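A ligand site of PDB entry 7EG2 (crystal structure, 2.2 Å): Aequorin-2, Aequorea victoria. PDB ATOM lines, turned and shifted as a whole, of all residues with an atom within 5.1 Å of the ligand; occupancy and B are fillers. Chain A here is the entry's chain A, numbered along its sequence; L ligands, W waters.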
ATOM      1  N   HIS A  25      -0.711  -7.655  18.548  1.00  0.00           N
ATOM      2  CA  HIS A  25      -1.419  -8.655  17.766  1.00  0.00           C
ATOM      3  C   HIS A  25      -2.367  -8.039  16.743  1.00  0.00           C
ATOM      4  O   HIS A  25      -2.684  -8.686  15.750  1.00  0.00           O
ATOM      5  CB  HIS A  25      -2.182  -9.595  18.695  1.00  0.00           C
ATOM      6  CG  HIS A  25      -1.285 -10.425  19.567  1.00  0.00           C
ATOM      7  ND1 HIS A  25      -0.493 -11.432  19.073  1.00  0.00           N
ATOM      8  CD2 HIS A  25      -1.045 -10.370  20.903  1.00  0.00           C
ATOM      9  CE1 HIS A  25       0.188 -11.981  20.061  1.00  0.00           C
ATOM     10  NE2 HIS A  25      -0.125 -11.352  21.189  1.00  0.00           N
ATOM     11  N   MET A  28      -0.129  -7.666  13.935  1.00  0.00           N
ATOM     12  CA  MET A  28       0.019  -8.970  13.286  1.00  0.00           C
ATOM     13  C   MET A  28      -1.234  -9.341  12.501  1.00  0.00           C
ATOM     14  O   MET A  28      -1.138  -9.918  11.413  1.00  0.00           O
ATOM     15  CB  MET A  28       0.330 -10.042  14.335  1.00  0.00           C
ATOM     16  CG  MET A  28       1.684  -9.863  15.013  1.00  0.00           C
ATOM     17  SD  MET A  28       3.054  -9.761  13.841  1.00  0.00           S
ATOM     18  CE  MET A  28       2.890 -11.315  12.970  1.00  0.00           C
ATOM     19  N   PHE A  29      -2.418  -9.011  13.041  1.00  0.00           N
ATOM     20  CA  PHE A  29      -3.656  -9.299  12.323  1.00  0.00           C
ATOM     21  C   PHE A  29      -3.704  -8.574  10.991  1.00  0.00           C
ATOM     22  O   PHE A  29      -4.010  -9.180   9.946  1.00  0.00           O
ATOM     23  CB  PHE A  29      -4.865  -8.917  13.190  1.00  0.00           C
ATOM     24  CG  PHE A  29      -6.193  -9.176  12.532  1.00  0.00           C
ATOM     25  CD1 PHE A  29      -6.822 -10.396  12.677  1.00  0.00           C
ATOM     26  CD2 PHE A  29      -6.814  -8.191  11.787  1.00  0.00           C
ATOM     27  CE1 PHE A  29      -8.048 -10.640  12.075  1.00  0.00           C
ATOM     28  CE2 PHE A  29      -8.032  -8.423  11.184  1.00  0.00           C
ATOM     29  CZ  PHE A  29      -8.661  -9.643  11.330  1.00  0.00           C
ATOM     30  N   PHE A  31      -1.203  -7.544   9.351  1.00  0.00           N
ATOM     31  CA  PHE A  31      -0.158  -8.131   8.504  1.00  0.00           C
ATOM     32  C   PHE A  31      -0.627  -9.427   7.861  1.00  0.00           C
ATOM     33  O   PHE A  31      -0.254  -9.720   6.719  1.00  0.00           O
ATOM     34  CB  PHE A  31       1.108  -8.371   9.338  1.00  0.00           C
ATOM     35  CG  PHE A  31       2.043  -9.370   8.745  1.00  0.00           C
ATOM     36  CD1 PHE A  31       2.815  -9.056   7.636  1.00  0.00           C
ATOM     37  CD2 PHE A  31       2.168 -10.633   9.297  1.00  0.00           C
ATOM     38  CE1 PHE A  31       3.680  -9.989   7.091  1.00  0.00           C
ATOM     39  CE2 PHE A  31       3.037 -11.570   8.760  1.00  0.00           C
ATOM     40  CZ  PHE A  31       3.795 -11.245   7.651  1.00  0.00           C
ATOM     41  N   LEU A  32      -1.441 -10.213   8.561  1.00  0.00           N
ATOM     42  CA  LEU A  32      -1.952 -11.460   8.017  1.00  0.00           C
ATOM     43  C   LEU A  32      -3.136 -11.255   7.080  1.00  0.00           C
ATOM     44  O   LEU A  32      -3.406 -12.112   6.238  1.00  0.00           O
ATOM     45  CB  LEU A  32      -2.357 -12.408   9.152  1.00  0.00           C
ATOM     46  CG  LEU A  32      -1.227 -12.839  10.091  1.00  0.00           C
ATOM     47  CD1 LEU A  32      -1.777 -13.619  11.279  1.00  0.00           C
ATOM     48  CD2 LEU A  32      -0.183 -13.649   9.336  1.00  0.00           C
ATOM     49  N   MET A  45      -3.752 -19.184   6.747  1.00  0.00           N
ATOM     50  CA  MET A  45      -2.566 -19.194   7.583  1.00  0.00           C
ATOM     51  C   MET A  45      -1.700 -20.411   7.298  1.00  0.00           C
ATOM     52  O   MET A  45      -0.482 -20.291   7.140  1.00  0.00           O
ATOM     53  CB  MET A  45      -2.965 -19.158   9.057  1.00  0.00           C
ATOM     54  CG  MET A  45      -3.800 -17.938   9.457  1.00  0.00           C
ATOM     55  SD  MET A  45      -2.920 -16.378   9.277  1.00  0.00           S
ATOM     56  CE  MET A  45      -3.559 -15.773   7.715  1.00  0.00           C
ATOM     57  N   LYS A  48      -0.078 -20.067   3.794  1.00  0.00           N
ATOM     58  CA  LYS A  48       1.090 -19.196   3.879  1.00  0.00           C
ATOM     59  C   LYS A  48       2.266 -19.928   4.502  1.00  0.00           C
ATOM     60  O   LYS A  48       3.388 -19.887   3.990  1.00  0.00           O
ATOM     61  CB  LYS A  48       0.751 -17.940   4.674  1.00  0.00           C
ATOM     62  CG  LYS A  48       1.908 -16.988   4.887  1.00  0.00           C
ATOM     63  CD  LYS A  48       1.585 -15.972   5.972  1.00  0.00           C
ATOM     64  CE  LYS A  48       2.738 -15.013   6.226  1.00  0.00           C
ATOM     65  NZ  LYS A  48       2.872 -13.998   5.142  1.00  0.00           N
ATOM     66  N   ALA A  49       2.026 -20.620   5.621  1.00  0.00           N
ATOM     67  CA  ALA A  49       3.102 -21.303   6.339  1.00  0.00           C
ATOM     68  C   ALA A  49       3.748 -22.379   5.485  1.00  0.00           C
ATOM     69  O   ALA A  49       4.973 -22.464   5.397  1.00  0.00           O
ATOM     70  CB  ALA A  49       2.555 -21.898   7.634  1.00  0.00           C
ATOM     71  N   ILE A  52       5.786 -21.022   2.367  1.00  0.00           N
ATOM     72  CA  ILE A  52       7.119 -20.502   2.648  1.00  0.00           C
ATOM     73  C   ILE A  52       8.139 -21.631   2.701  1.00  0.00           C
ATOM     74  O   ILE A  52       9.167 -21.595   2.013  1.00  0.00           O
ATOM     75  CB  ILE A  52       7.114 -19.708   3.973  1.00  0.00           C
ATOM     76  CG1 ILE A  52       6.185 -18.492   3.865  1.00  0.00           C
ATOM     77  CG2 ILE A  52       8.525 -19.251   4.321  1.00  0.00           C
ATOM     78  CD1 ILE A  52       5.763 -17.941   5.204  1.00  0.00           C
ATOM     79  N   VAL A  71       1.942 -25.473  12.686  1.00  0.00           N
ATOM     80  CA  VAL A  71       1.254 -24.212  12.415  1.00  0.00           C
ATOM     81  C   VAL A  71      -0.253 -24.376  12.609  1.00  0.00           C
ATOM     82  O   VAL A  71      -0.924 -23.509  13.180  1.00  0.00           O
ATOM     83  CB  VAL A  71       1.585 -23.711  11.004  1.00  0.00           C
ATOM     84  CG1 VAL A  71       0.951 -22.346  10.774  1.00  0.00           C
ATOM     85  CG2 VAL A  71       3.078 -23.654  10.782  1.00  0.00           C
ATOM     86  N   PHE A  74      -1.044 -24.273  16.133  1.00  0.00           N
ATOM     87  CA  PHE A  74      -0.790 -22.960  16.708  1.00  0.00           C
ATOM     88  C   PHE A  74      -1.978 -22.027  16.503  1.00  0.00           C
ATOM     89  O   PHE A  74      -2.594 -21.563  17.467  1.00  0.00           O
ATOM     90  CB  PHE A  74       0.486 -22.367  16.119  1.00  0.00           C
ATOM     91  CG  PHE A  74       0.842 -21.019  16.663  1.00  0.00           C
ATOM     92  CD1 PHE A  74       1.423 -20.892  17.920  1.00  0.00           C
ATOM     93  CD2 PHE A  74       0.609 -19.865  15.931  1.00  0.00           C
ATOM     94  CE1 PHE A  74       1.751 -19.650  18.432  1.00  0.00           C
ATOM     95  CE2 PHE A  74       0.932 -18.620  16.434  1.00  0.00           C
ATOM     96  CZ  PHE A  74       1.505 -18.514  17.689  1.00  0.00           C
ATOM     97  N   PHE A  75      -2.310 -21.739  15.238  1.00  0.00           N
ATOM     98  CA  PHE A  75      -3.438 -20.856  14.971  1.00  0.00           C
ATOM     99  C   PHE A  75      -4.762 -21.490  15.371  1.00  0.00           C
ATOM    100  O   PHE A  75      -5.723 -20.778  15.692  1.00  0.00           O
ATOM    101  CB  PHE A  75      -3.456 -20.459  13.490  1.00  0.00           C
ATOM    102  CG  PHE A  75      -2.343 -19.529  13.103  1.00  0.00           C
ATOM    103  CD1 PHE A  75      -2.431 -18.176  13.379  1.00  0.00           C
ATOM    104  CD2 PHE A  75      -1.199 -20.013  12.485  1.00  0.00           C
ATOM    105  CE1 PHE A  75      -1.401 -17.314  13.026  1.00  0.00           C
ATOM    106  CE2 PHE A  75      -0.168 -19.151  12.132  1.00  0.00           C
ATOM    107  CZ  PHE A  75      -0.278 -17.808  12.405  1.00  0.00           C
ATOM    108  N   TYR A  91     -10.619 -12.747  16.807  1.00  0.00           N
ATOM    109  CA  TYR A  91      -9.185 -13.053  16.733  1.00  0.00           C
ATOM    110  C   TYR A  91      -8.502 -12.747  18.067  1.00  0.00           C
ATOM    111  O   TYR A  91      -7.849 -13.626  18.663  1.00  0.00           O
ATOM    112  CB  TYR A  91      -8.542 -12.259  15.607  1.00  0.00           C
ATOM    113  CG  TYR A  91      -7.065 -12.516  15.431  1.00  0.00           C
ATOM    114  CD1 TYR A  91      -6.611 -13.580  14.674  1.00  0.00           C
ATOM    115  CD2 TYR A  91      -6.123 -11.673  16.021  1.00  0.00           C
ATOM    116  CE1 TYR A  91      -5.256 -13.815  14.512  1.00  0.00           C
ATOM    117  CE2 TYR A  91      -4.768 -11.899  15.863  1.00  0.00           C
ATOM    118  CZ  TYR A  91      -4.346 -12.975  15.106  1.00  0.00           C
ATOM    119  OH  TYR A  91      -3.000 -13.202  14.952  1.00  0.00           O
ATOM    120  N   TRP A  95      -6.838 -15.133  20.859  1.00  0.00           N
ATOM    121  CA  TRP A  95      -5.432 -15.024  21.260  1.00  0.00           C
ATOM    122  C   TRP A  95      -5.292 -14.941  22.777  1.00  0.00           C
ATOM    123  O   TRP A  95      -4.232 -15.306  23.313  1.00  0.00           O
ATOM    124  CB  TRP A  95      -4.781 -13.818  20.587  1.00  0.00           C
ATOM    125  CG  TRP A  95      -3.783 -14.214  19.557  1.00  0.00           C
ATOM    126  CD1 TRP A  95      -3.982 -14.283  18.206  1.00  0.00           C
ATOM    127  CD2 TRP A  95      -2.430 -14.630  19.787  1.00  0.00           C
ATOM    128  NE1 TRP A  95      -2.835 -14.699  17.575  1.00  0.00           N
ATOM    129  CE2 TRP A  95      -1.865 -14.918  18.529  1.00  0.00           C
ATOM    130  CE3 TRP A  95      -1.646 -14.782  20.923  1.00  0.00           C
ATOM    131  CZ2 TRP A  95      -0.552 -15.351  18.383  1.00  0.00           C
ATOM    132  CZ3 TRP A  95      -0.343 -15.207  20.785  1.00  0.00           C
ATOM    133  CH2 TRP A  95       0.195 -15.484  19.523  1.00  0.00           C
ATOM    134  N   ILE A 114       4.157 -22.917  20.490  1.00  0.00           N
ATOM    135  CA  ILE A 114       5.143 -22.071  19.848  1.00  0.00           C
ATOM    136  C   ILE A 114       6.493 -22.786  19.753  1.00  0.00           C
ATOM    137  O   ILE A 114       7.264 -22.555  18.819  1.00  0.00           O
ATOM    138  CB  ILE A 114       5.248 -20.722  20.575  1.00  0.00           C
ATOM    139  CG1 ILE A 114       6.059 -19.721  19.748  1.00  0.00           C
ATOM    140  CG2 ILE A 114       5.863 -20.895  21.963  1.00  0.00           C
ATOM    141  CD1 ILE A 114       5.396 -19.326  18.449  1.00  0.00           C
ATOM    142  N   TRP A 117       6.213 -25.506  16.858  1.00  0.00           N
ATOM    143  CA  TRP A 117       6.377 -24.832  15.572  1.00  0.00           C
ATOM    144  C   TRP A 117       7.832 -24.482  15.326  1.00  0.00           C
ATOM    145  O   TRP A 117       8.348 -24.651  14.207  1.00  0.00           O
ATOM    146  CB  TRP A 117       5.492 -23.592  15.519  1.00  0.00           C
ATOM    147  CG  TRP A 117       5.467 -22.894  14.177  1.00  0.00           C
ATOM    148  CD1 TRP A 117       5.980 -23.350  12.998  1.00  0.00           C
ATOM    149  CD2 TRP A 117       4.916 -21.605  13.900  1.00  0.00           C
ATOM    150  NE1 TRP A 117       5.773 -22.433  12.007  1.00  0.00           N
ATOM    151  CE2 TRP A 117       5.122 -21.344  12.524  1.00  0.00           C
ATOM    152  CE3 TRP A 117       4.265 -20.639  14.672  1.00  0.00           C
ATOM    153  CZ2 TRP A 117       4.696 -20.167  11.916  1.00  0.00           C
ATOM    154  CZ3 TRP A 117       3.848 -19.469  14.057  1.00  0.00           C
ATOM    155  CH2 TRP A 117       4.064 -19.242  12.688  1.00  0.00           C
ATOM    156  N   GLY A 118       8.527 -23.986  16.361  1.00  0.00           N
ATOM    157  CA  GLY A 118       9.923 -23.620  16.189  1.00  0.00           C
ATOM    158  C   GLY A 118      10.802 -24.816  15.845  1.00  0.00           C
ATOM    159  O   GLY A 118      11.667 -24.732  14.976  1.00  0.00           O
ATOM    160  N   LEU A 121      10.066 -25.789  12.288  1.00  0.00           N
ATOM    161  CA  LEU A 121      10.555 -24.782  11.352  1.00  0.00           C
ATOM    162  C   LEU A 121      12.070 -24.737  11.316  1.00  0.00           C
ATOM    163  O   LEU A 121      12.662 -24.659  10.226  1.00  0.00           O
ATOM    164  CB  LEU A 121       9.987 -23.404  11.719  1.00  0.00           C
ATOM    165  CG  LEU A 121      10.479 -22.263  10.827  1.00  0.00           C
ATOM    166  CD1 LEU A 121      10.076 -22.496   9.378  1.00  0.00           C
ATOM    167  CD2 LEU A 121       9.936 -20.928  11.320  1.00  0.00           C
ATOM    168  N   PHE A 122      12.721 -24.786  12.477  1.00  0.00           N
ATOM    169  CA  PHE A 122      14.176 -24.681  12.505  1.00  0.00           C
ATOM    170  C   PHE A 122      14.845 -25.892  11.855  1.00  0.00           C
ATOM    171  O   PHE A 122      15.945 -25.757  11.315  1.00  0.00           O
ATOM    172  CB  PHE A 122      14.676 -24.514  13.939  1.00  0.00           C
ATOM    173  CG  PHE A 122      14.710 -23.080  14.389  1.00  0.00           C
ATOM    174  CD1 PHE A 122      13.836 -22.144  13.849  1.00  0.00           C
ATOM    175  CD2 PHE A 122      15.622 -22.657  15.353  1.00  0.00           C
ATOM    176  CE1 PHE A 122      13.866 -20.825  14.263  1.00  0.00           C
ATOM    177  CE2 PHE A 122      15.651 -21.338  15.767  1.00  0.00           C
ATOM    178  CZ  PHE A 122      14.778 -20.421  15.220  1.00  0.00           C
ATOM    179  N   TRP A 138      17.953 -16.673   9.453  1.00  0.00           N
ATOM    180  CA  TRP A 138      16.857 -15.932  10.070  1.00  0.00           C
ATOM    181  C   TRP A 138      16.383 -14.804   9.176  1.00  0.00           C
ATOM    182  O   TRP A 138      15.183 -14.508   9.120  1.00  0.00           O
ATOM    183  CB  TRP A 138      17.304 -15.391  11.433  1.00  0.00           C
ATOM    184  CG  TRP A 138      16.302 -14.512  12.117  1.00  0.00           C
ATOM    185  CD1 TRP A 138      16.424 -13.170  12.358  1.00  0.00           C
ATOM    186  CD2 TRP A 138      15.035 -14.894  12.652  1.00  0.00           C
ATOM    187  NE1 TRP A 138      15.312 -12.708  13.010  1.00  0.00           N
ATOM    188  CE2 TRP A 138      14.445 -13.751  13.202  1.00  0.00           C
ATOM    189  CE3 TRP A 138      14.344 -16.109  12.715  1.00  0.00           C
ATOM    190  CZ2 TRP A 138      13.188 -13.770  13.818  1.00  0.00           C
ATOM    191  CZ3 TRP A 138      13.097 -16.135  13.324  1.00  0.00           C
ATOM    192  CH2 TRP A 138      12.532 -14.967  13.867  1.00  0.00           C
ATOM    193  N   TYR A 141      14.170 -16.500   6.344  1.00  0.00           N
ATOM    194  CA  TYR A 141      12.805 -16.885   6.695  1.00  0.00           C
ATOM    195  C   TYR A 141      11.916 -15.665   6.910  1.00  0.00           C
ATOM    196  O   TYR A 141      10.830 -15.577   6.343  1.00  0.00           O
ATOM    197  CB  TYR A 141      12.774 -17.780   7.930  1.00  0.00           C
ATOM    198  CG  TYR A 141      11.362 -18.087   8.356  1.00  0.00           C
ATOM    199  CD1 TYR A 141      10.602 -19.024   7.659  1.00  0.00           C
ATOM    200  CD2 TYR A 141      10.765 -17.408   9.406  1.00  0.00           C
ATOM    201  CE1 TYR A 141       9.301 -19.295   8.025  1.00  0.00           C
ATOM    202  CE2 TYR A 141       9.454 -17.681   9.776  1.00  0.00           C
ATOM    203  CZ  TYR A 141       8.727 -18.624   9.072  1.00  0.00           C
ATOM    204  OH  TYR A 141       7.430 -18.900   9.422  1.00  0.00           O
ATOM    205  N   THR A 142      12.371 -14.726   7.749  1.00  0.00           N
ATOM    206  CA  THR A 142      11.508 -13.610   8.141  1.00  0.00           C
ATOM    207  C   THR A 142      11.164 -12.718   6.966  1.00  0.00           C
ATOM    208  O   THR A 142      10.061 -12.157   6.922  1.00  0.00           O
ATOM    209  CB  THR A 142      12.174 -12.802   9.249  1.00  0.00           C
ATOM    210  OG1 THR A 142      13.450 -12.331   8.797  1.00  0.00           O
ATOM    211  CG2 THR A 142      12.360 -13.658  10.485  1.00  0.00           C
ATOM    212  N   ALA A 145       8.618 -14.763   4.875  1.00  0.00           N
ATOM    213  CA  ALA A 145       7.315 -14.627   5.532  1.00  0.00           C
ATOM    214  C   ALA A 145       6.835 -13.183   5.542  1.00  0.00           C
ATOM    215  O   ALA A 145       5.627 -12.935   5.592  1.00  0.00           O
ATOM    216  CB  ALA A 145       7.384 -15.174   6.960  1.00  0.00           C
ATOM    217  N   ILE A 147       7.360 -11.051   7.965  1.00  0.00           N
ATOM    218  CA  ILE A 147       7.189 -10.530   9.323  1.00  0.00           C
ATOM    219  C   ILE A 147       8.277  -9.516   9.654  1.00  0.00           C
ATOM    220  O   ILE A 147       8.066  -8.614  10.474  1.00  0.00           O
ATOM    221  CB  ILE A 147       7.140 -11.687  10.337  1.00  0.00           C
ATOM    222  CG1 ILE A 147       6.733 -11.171  11.716  1.00  0.00           C
ATOM    223  CG2 ILE A 147       8.477 -12.416  10.400  1.00  0.00           C
ATOM    224  CD1 ILE A 147       6.521 -12.265  12.745  1.00  0.00           C
ATOM    225  N   VAL A 171      15.889 -23.134  19.271  1.00  0.00           N
ATOM    226  CA  VAL A 171      14.476 -23.045  19.628  1.00  0.00           C
ATOM    227  C   VAL A 171      14.314 -22.760  21.116  1.00  0.00           C
ATOM    228  O   VAL A 171      13.355 -22.078  21.522  1.00  0.00           O
ATOM    229  CB  VAL A 171      13.729 -24.325  19.213  1.00  0.00           C
ATOM    230  CG1 VAL A 171      12.263 -24.247  19.596  1.00  0.00           C
ATOM    231  CG2 VAL A 171      13.881 -24.556  17.725  1.00  0.00           C
ATOM    232  N   MET A 174      14.624 -18.981  21.444  1.00  0.00           N
ATOM    233  CA  MET A 174      13.526 -18.285  20.779  1.00  0.00           C
ATOM    234  C   MET A 174      12.201 -18.539  21.484  1.00  0.00           C
ATOM    235  O   MET A 174      11.342 -17.649  21.525  1.00  0.00           O
ATOM    236  CB  MET A 174      13.434 -18.712  19.310  1.00  0.00           C
ATOM    237  CG  MET A 174      12.691 -17.707  18.437  1.00  0.00           C
ATOM    238  SD  MET A 174      13.376 -16.050  18.622  1.00  0.00           S
ATOM    239  CE  MET A 174      12.486 -15.178  17.333  1.00  0.00           C
ATOM    240  N   THR A 175      12.011 -19.740  22.039  1.00  0.00           N
ATOM    241  CA  THR A 175      10.821 -19.998  22.859  1.00  0.00           C
ATOM    242  C   THR A 175      10.827 -19.147  24.114  1.00  0.00           C
ATOM    243  O   THR A 175       9.764 -18.702  24.579  1.00  0.00           O
ATOM    244  CB  THR A 175      10.739 -21.475  23.215  1.00  0.00           C
ATOM    245  OG1 THR A 175      10.905 -22.273  22.038  1.00  0.00           O
ATOM    246  CG2 THR A 175       9.390 -21.806  23.836  1.00  0.00           C
ATOM    247  N   HIS A 178       9.913 -15.675  22.821  1.00  0.00           N
ATOM    248  CA  HIS A 178       8.515 -15.623  22.387  1.00  0.00           C
ATOM    249  C   HIS A 178       7.550 -15.688  23.553  1.00  0.00           C
ATOM    250  O   HIS A 178       6.415 -15.204  23.453  1.00  0.00           O
ATOM    251  CB  HIS A 178       8.227 -16.746  21.395  1.00  0.00           C
ATOM    252  CG  HIS A 178       8.637 -16.438  19.995  1.00  0.00           C
ATOM    253  ND1 HIS A 178       8.819 -17.417  19.034  1.00  0.00           N
ATOM    254  CD2 HIS A 178       8.891 -15.264  19.373  1.00  0.00           C
ATOM    255  CE1 HIS A 178       9.166 -16.853  17.896  1.00  0.00           C
ATOM    256  NE2 HIS A 178       9.223 -15.546  18.078  1.00  0.00           N
ATOM    257  N   TRP A 182       5.130 -12.539  22.695  1.00  0.00           N
ATOM    258  CA  TRP A 182       3.770 -12.785  22.236  1.00  0.00           C
ATOM    259  C   TRP A 182       2.759 -12.924  23.367  1.00  0.00           C
ATOM    260  O   TRP A 182       1.581 -12.630  23.168  1.00  0.00           O
ATOM    261  CB  TRP A 182       3.707 -14.052  21.371  1.00  0.00           C
ATOM    262  CG  TRP A 182       4.525 -14.017  20.097  1.00  0.00           C
ATOM    263  CD1 TRP A 182       5.421 -14.955  19.687  1.00  0.00           C
ATOM    264  CD2 TRP A 182       4.498 -12.999  19.077  1.00  0.00           C
ATOM    265  NE1 TRP A 182       5.963 -14.590  18.472  1.00  0.00           N
ATOM    266  CE2 TRP A 182       5.411 -13.399  18.080  1.00  0.00           C
ATOM    267  CE3 TRP A 182       3.793 -11.807  18.910  1.00  0.00           C
ATOM    268  CZ2 TRP A 182       5.648 -12.635  16.938  1.00  0.00           C
ATOM    269  CZ3 TRP A 182       4.026 -11.049  17.781  1.00  0.00           C
ATOM    270  CH2 TRP A 182       4.945 -11.468  16.809  1.00  0.00           C
ATOM    271  N   TYR A 193      11.815  -8.321  17.387  1.00  0.00           N
ATOM    272  CA  TYR A 193      11.722  -8.212  15.932  1.00  0.00           C
ATOM    273  C   TYR A 193      12.143  -6.835  15.442  1.00  0.00           C
ATOM    274  O   TYR A 193      11.725  -6.395  14.369  1.00  0.00           O
ATOM    275  CB  TYR A 193      10.301  -8.546  15.476  1.00  0.00           C
ATOM    276  CG  TYR A 193       9.959 -10.013  15.597  1.00  0.00           C
ATOM    277  CD1 TYR A 193       9.593 -10.556  16.823  1.00  0.00           C
ATOM    278  CD2 TYR A 193      10.011 -10.851  14.493  1.00  0.00           C
ATOM    279  CE1 TYR A 193       9.296 -11.905  16.947  1.00  0.00           C
ATOM    280  CE2 TYR A 193       9.709 -12.198  14.608  1.00  0.00           C
ATOM    281  CZ  TYR A 193       9.347 -12.717  15.828  1.00  0.00           C
ATOM    282  OH  TYR A 193       9.054 -14.052  15.943  1.00  0.00           O
HETATM  283  C1  LIG L   1      10.363 -19.194  14.884  1.00  0.00           C
HETATM  284  C2  LIG L   1       5.566 -16.144  12.722  1.00  0.00           C
HETATM  285  C3  LIG L   1       6.794 -16.860  12.230  1.00  0.00           C
HETATM  286  C4  LIG L   1       4.506 -15.540  12.052  1.00  0.00           C
HETATM  287  C5  LIG L   1       4.183 -15.380  10.609  1.00  0.00           C
HETATM  288  C6  LIG L   1       3.460 -16.472   9.876  1.00  0.00           C
HETATM  289  C7  LIG L   1       4.199 -17.492   9.263  1.00  0.00           C
HETATM  290  C8  LIG L   1       3.559 -18.528   8.587  1.00  0.00           C
HETATM  291  C9  LIG L   1       2.174 -18.566   8.496  1.00  0.00           C
HETATM  292  C10 LIG L   1       1.431 -17.561   9.093  1.00  0.00           C
HETATM  293  C11 LIG L   1       2.061 -16.518   9.777  1.00  0.00           C
HETATM  294  C12 LIG L   1       3.543 -14.990  12.890  1.00  0.00           C
HETATM  295  C13 LIG L   1       3.474 -14.937  14.262  1.00  0.00           C
HETATM  296  C14 LIG L   1       1.123 -14.267  14.173  1.00  0.00           C
HETATM  297  C15 LIG L   1      -0.030 -13.669  14.679  1.00  0.00           C
HETATM  298  C16 LIG L   1       0.002 -13.052  15.936  1.00  0.00           C
HETATM  299  C17 LIG L   1       1.201 -13.045  16.663  1.00  0.00           C
HETATM  300  C18 LIG L   1       2.337 -13.657  16.138  1.00  0.00           C
HETATM  301  C19 LIG L   1       6.743 -16.786  14.620  1.00  0.00           C
HETATM  302  C20 LIG L   1       7.696 -17.184  13.471  1.00  0.00           C
HETATM  303  C21 LIG L   1       9.019 -16.376  13.451  1.00  0.00           C
HETATM  304  C22 LIG L   1       8.245 -18.660  13.496  1.00  0.00           C
HETATM  305  C23 LIG L   1       8.967 -19.220  14.731  1.00  0.00           C
HETATM  306  C24 LIG L   1       8.241 -19.806  15.771  1.00  0.00           C
HETATM  307  C25 LIG L   1       8.855 -20.336  16.909  1.00  0.00           C
HETATM  308  C26 LIG L   1      10.245 -20.290  17.036  1.00  0.00           C
HETATM  309  C27 LIG L   1      11.003 -19.719  16.010  1.00  0.00           C
HETATM  310  C28 LIG L   1       5.588 -16.139  14.147  1.00  0.00           C
HETATM  311  C29 LIG L   1       4.551 -15.539  14.899  1.00  0.00           C
HETATM  312  C30 LIG L   1       2.332 -14.276  14.890  1.00  0.00           C
HETATM  313  O1  LIG L   1       7.043 -17.047  15.805  1.00  0.00           O
HETATM  314  O2  LIG L   1      10.845 -20.812  18.149  1.00  0.00           O
HETATM  315  O3  LIG L   1      -1.115 -12.455  16.446  1.00  0.00           O
HETATM  316  O4  LIG L   1       8.810 -15.000  13.409  1.00  0.00           O
HETATM  317  O   HOH W   1       9.379 -20.854  20.069  1.00  0.00           O
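A ring nitrogen (ND1) of His 25 is in hydrogen-bond range of an oxygen (O3) of the ligand (2.9 Å).
An oxygen (O3) of the ligand lies within hydrogen-bond range of the indole nitrogen of Trp 95.
The side-chain hydroxyl (OH) of Tyr 193 sits at hydrogen-bond distance from an oxygen (O4) of the ligand, at 2.7 Å.
O3 of the ligand sits at hydrogen-bond distance from OH of Tyr 91 (2.5 Å).
A ring nitrogen (NE2) of His 178 sits close to an oxygen (O1) of the ligand (3.5 Å).
O of Ala 145 lies within hydrogen-bond range of NZ of Lys 48 (3.0 Å).
The side-chain hydroxyl (OG1) of Thr 175 is in hydrogen-bond range of the backbone carbonyl oxygen (O) of Val 171, 2.5 Å away.
The backbone carbonyl oxygen (O) of Trp 138 lies within hydrogen-bond range of the side-chain hydroxyl (OG1) of Thr 142 (2.8 Å).
The side-chain hydroxyl (OH) of Tyr 193 lies within hydrogen-bond range of a ring nitrogen (NE2) of His 178, at 2.6 Å.
NE1 of Trp 182 lies close to NE2 of His 178, at 3.4 Å.
The side-chain hydroxyl (OH) of Tyr 91 is in hydrogen-bond range of the indole nitrogen (NE1) of Trp 95.
The backbone carbonyl oxygen (O) of Trp 182 is in hydrogen-bond range of a ring nitrogen (NE2) of His 25 (2.9 Å).
N of Ile 147 lies within hydrogen-bond range of O of Thr 142 (3.1 Å).
Met 28 touches the ligand (CB to C16, 3.4 Å).
CD2 of Leu 32 touches C11 of the ligand (3.7 Å).
O of Met 45 touches C9 of the ligand, at 3.4 Å.
Lys 48 touches the ligand (CD to C10, 3.5 Å).
Ala 49 touches the ligand (CB to C9, 3.5 Å).
CZ of Phe 75 touches C10 of the ligand, at 3.7 Å.
Ile 114 touches the ligand (O to C25, 3.3 Å).
CH2 of Trp 117 touches C2 of the ligand, 3.4 Å away.
Gly 118 touches the ligand.
Leu 121 touches the ligand.
CE1 of Phe 122 touches C27 of the ligand, 3.5 Å away.
Trp 138 touches the ligand (CH2 to O4, 3.8 Å).
OH of Tyr 141 touches C7 of the ligand, 3.5 Å away.
CD1 of Ile 147 touches O4 of the ligand (3.6 Å).
CG1 of Val 171 touches O2 of the ligand, at 3.99 Å.
Met 174 touches the ligand.
CH2 of Trp 182 touches C18 of the ligand, at 3.5 Å.
Hydrophobic or aromatic side chains that line the ligand: His 25, Met 28, Leu 32, Ala 49, Phe 75, Tyr 91, Trp 95, Ile 114, Trp 117, Leu 121, Phe 122, Trp 138, Tyr 141, Ile 147, Val 171, Met 174, His 178, Trp 182 and Tyr 193.
22 residues have an atom within 4 Å of the ligand: His 25, Met 28, Leu 32, Met 45, Lys 48, Ala 49, Phe 75, Tyr 91, Trp 95, Ile 114, Trp 117, Gly 118, Leu 121, Phe 122, Trp 138, Tyr 141, Ile 147, Val 171, Met 174, His 178, Trp 182 and Tyr 193.
The nearest printed residue that does not touch the ligand is Ile 52 (4.1 Å).
Water W1 lies within hydrogen-bond range of O2 of the ligand (2.4 Å), OG1 of Thr 175 (2.9 Å) and O of Ile 114 (3.0 Å).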
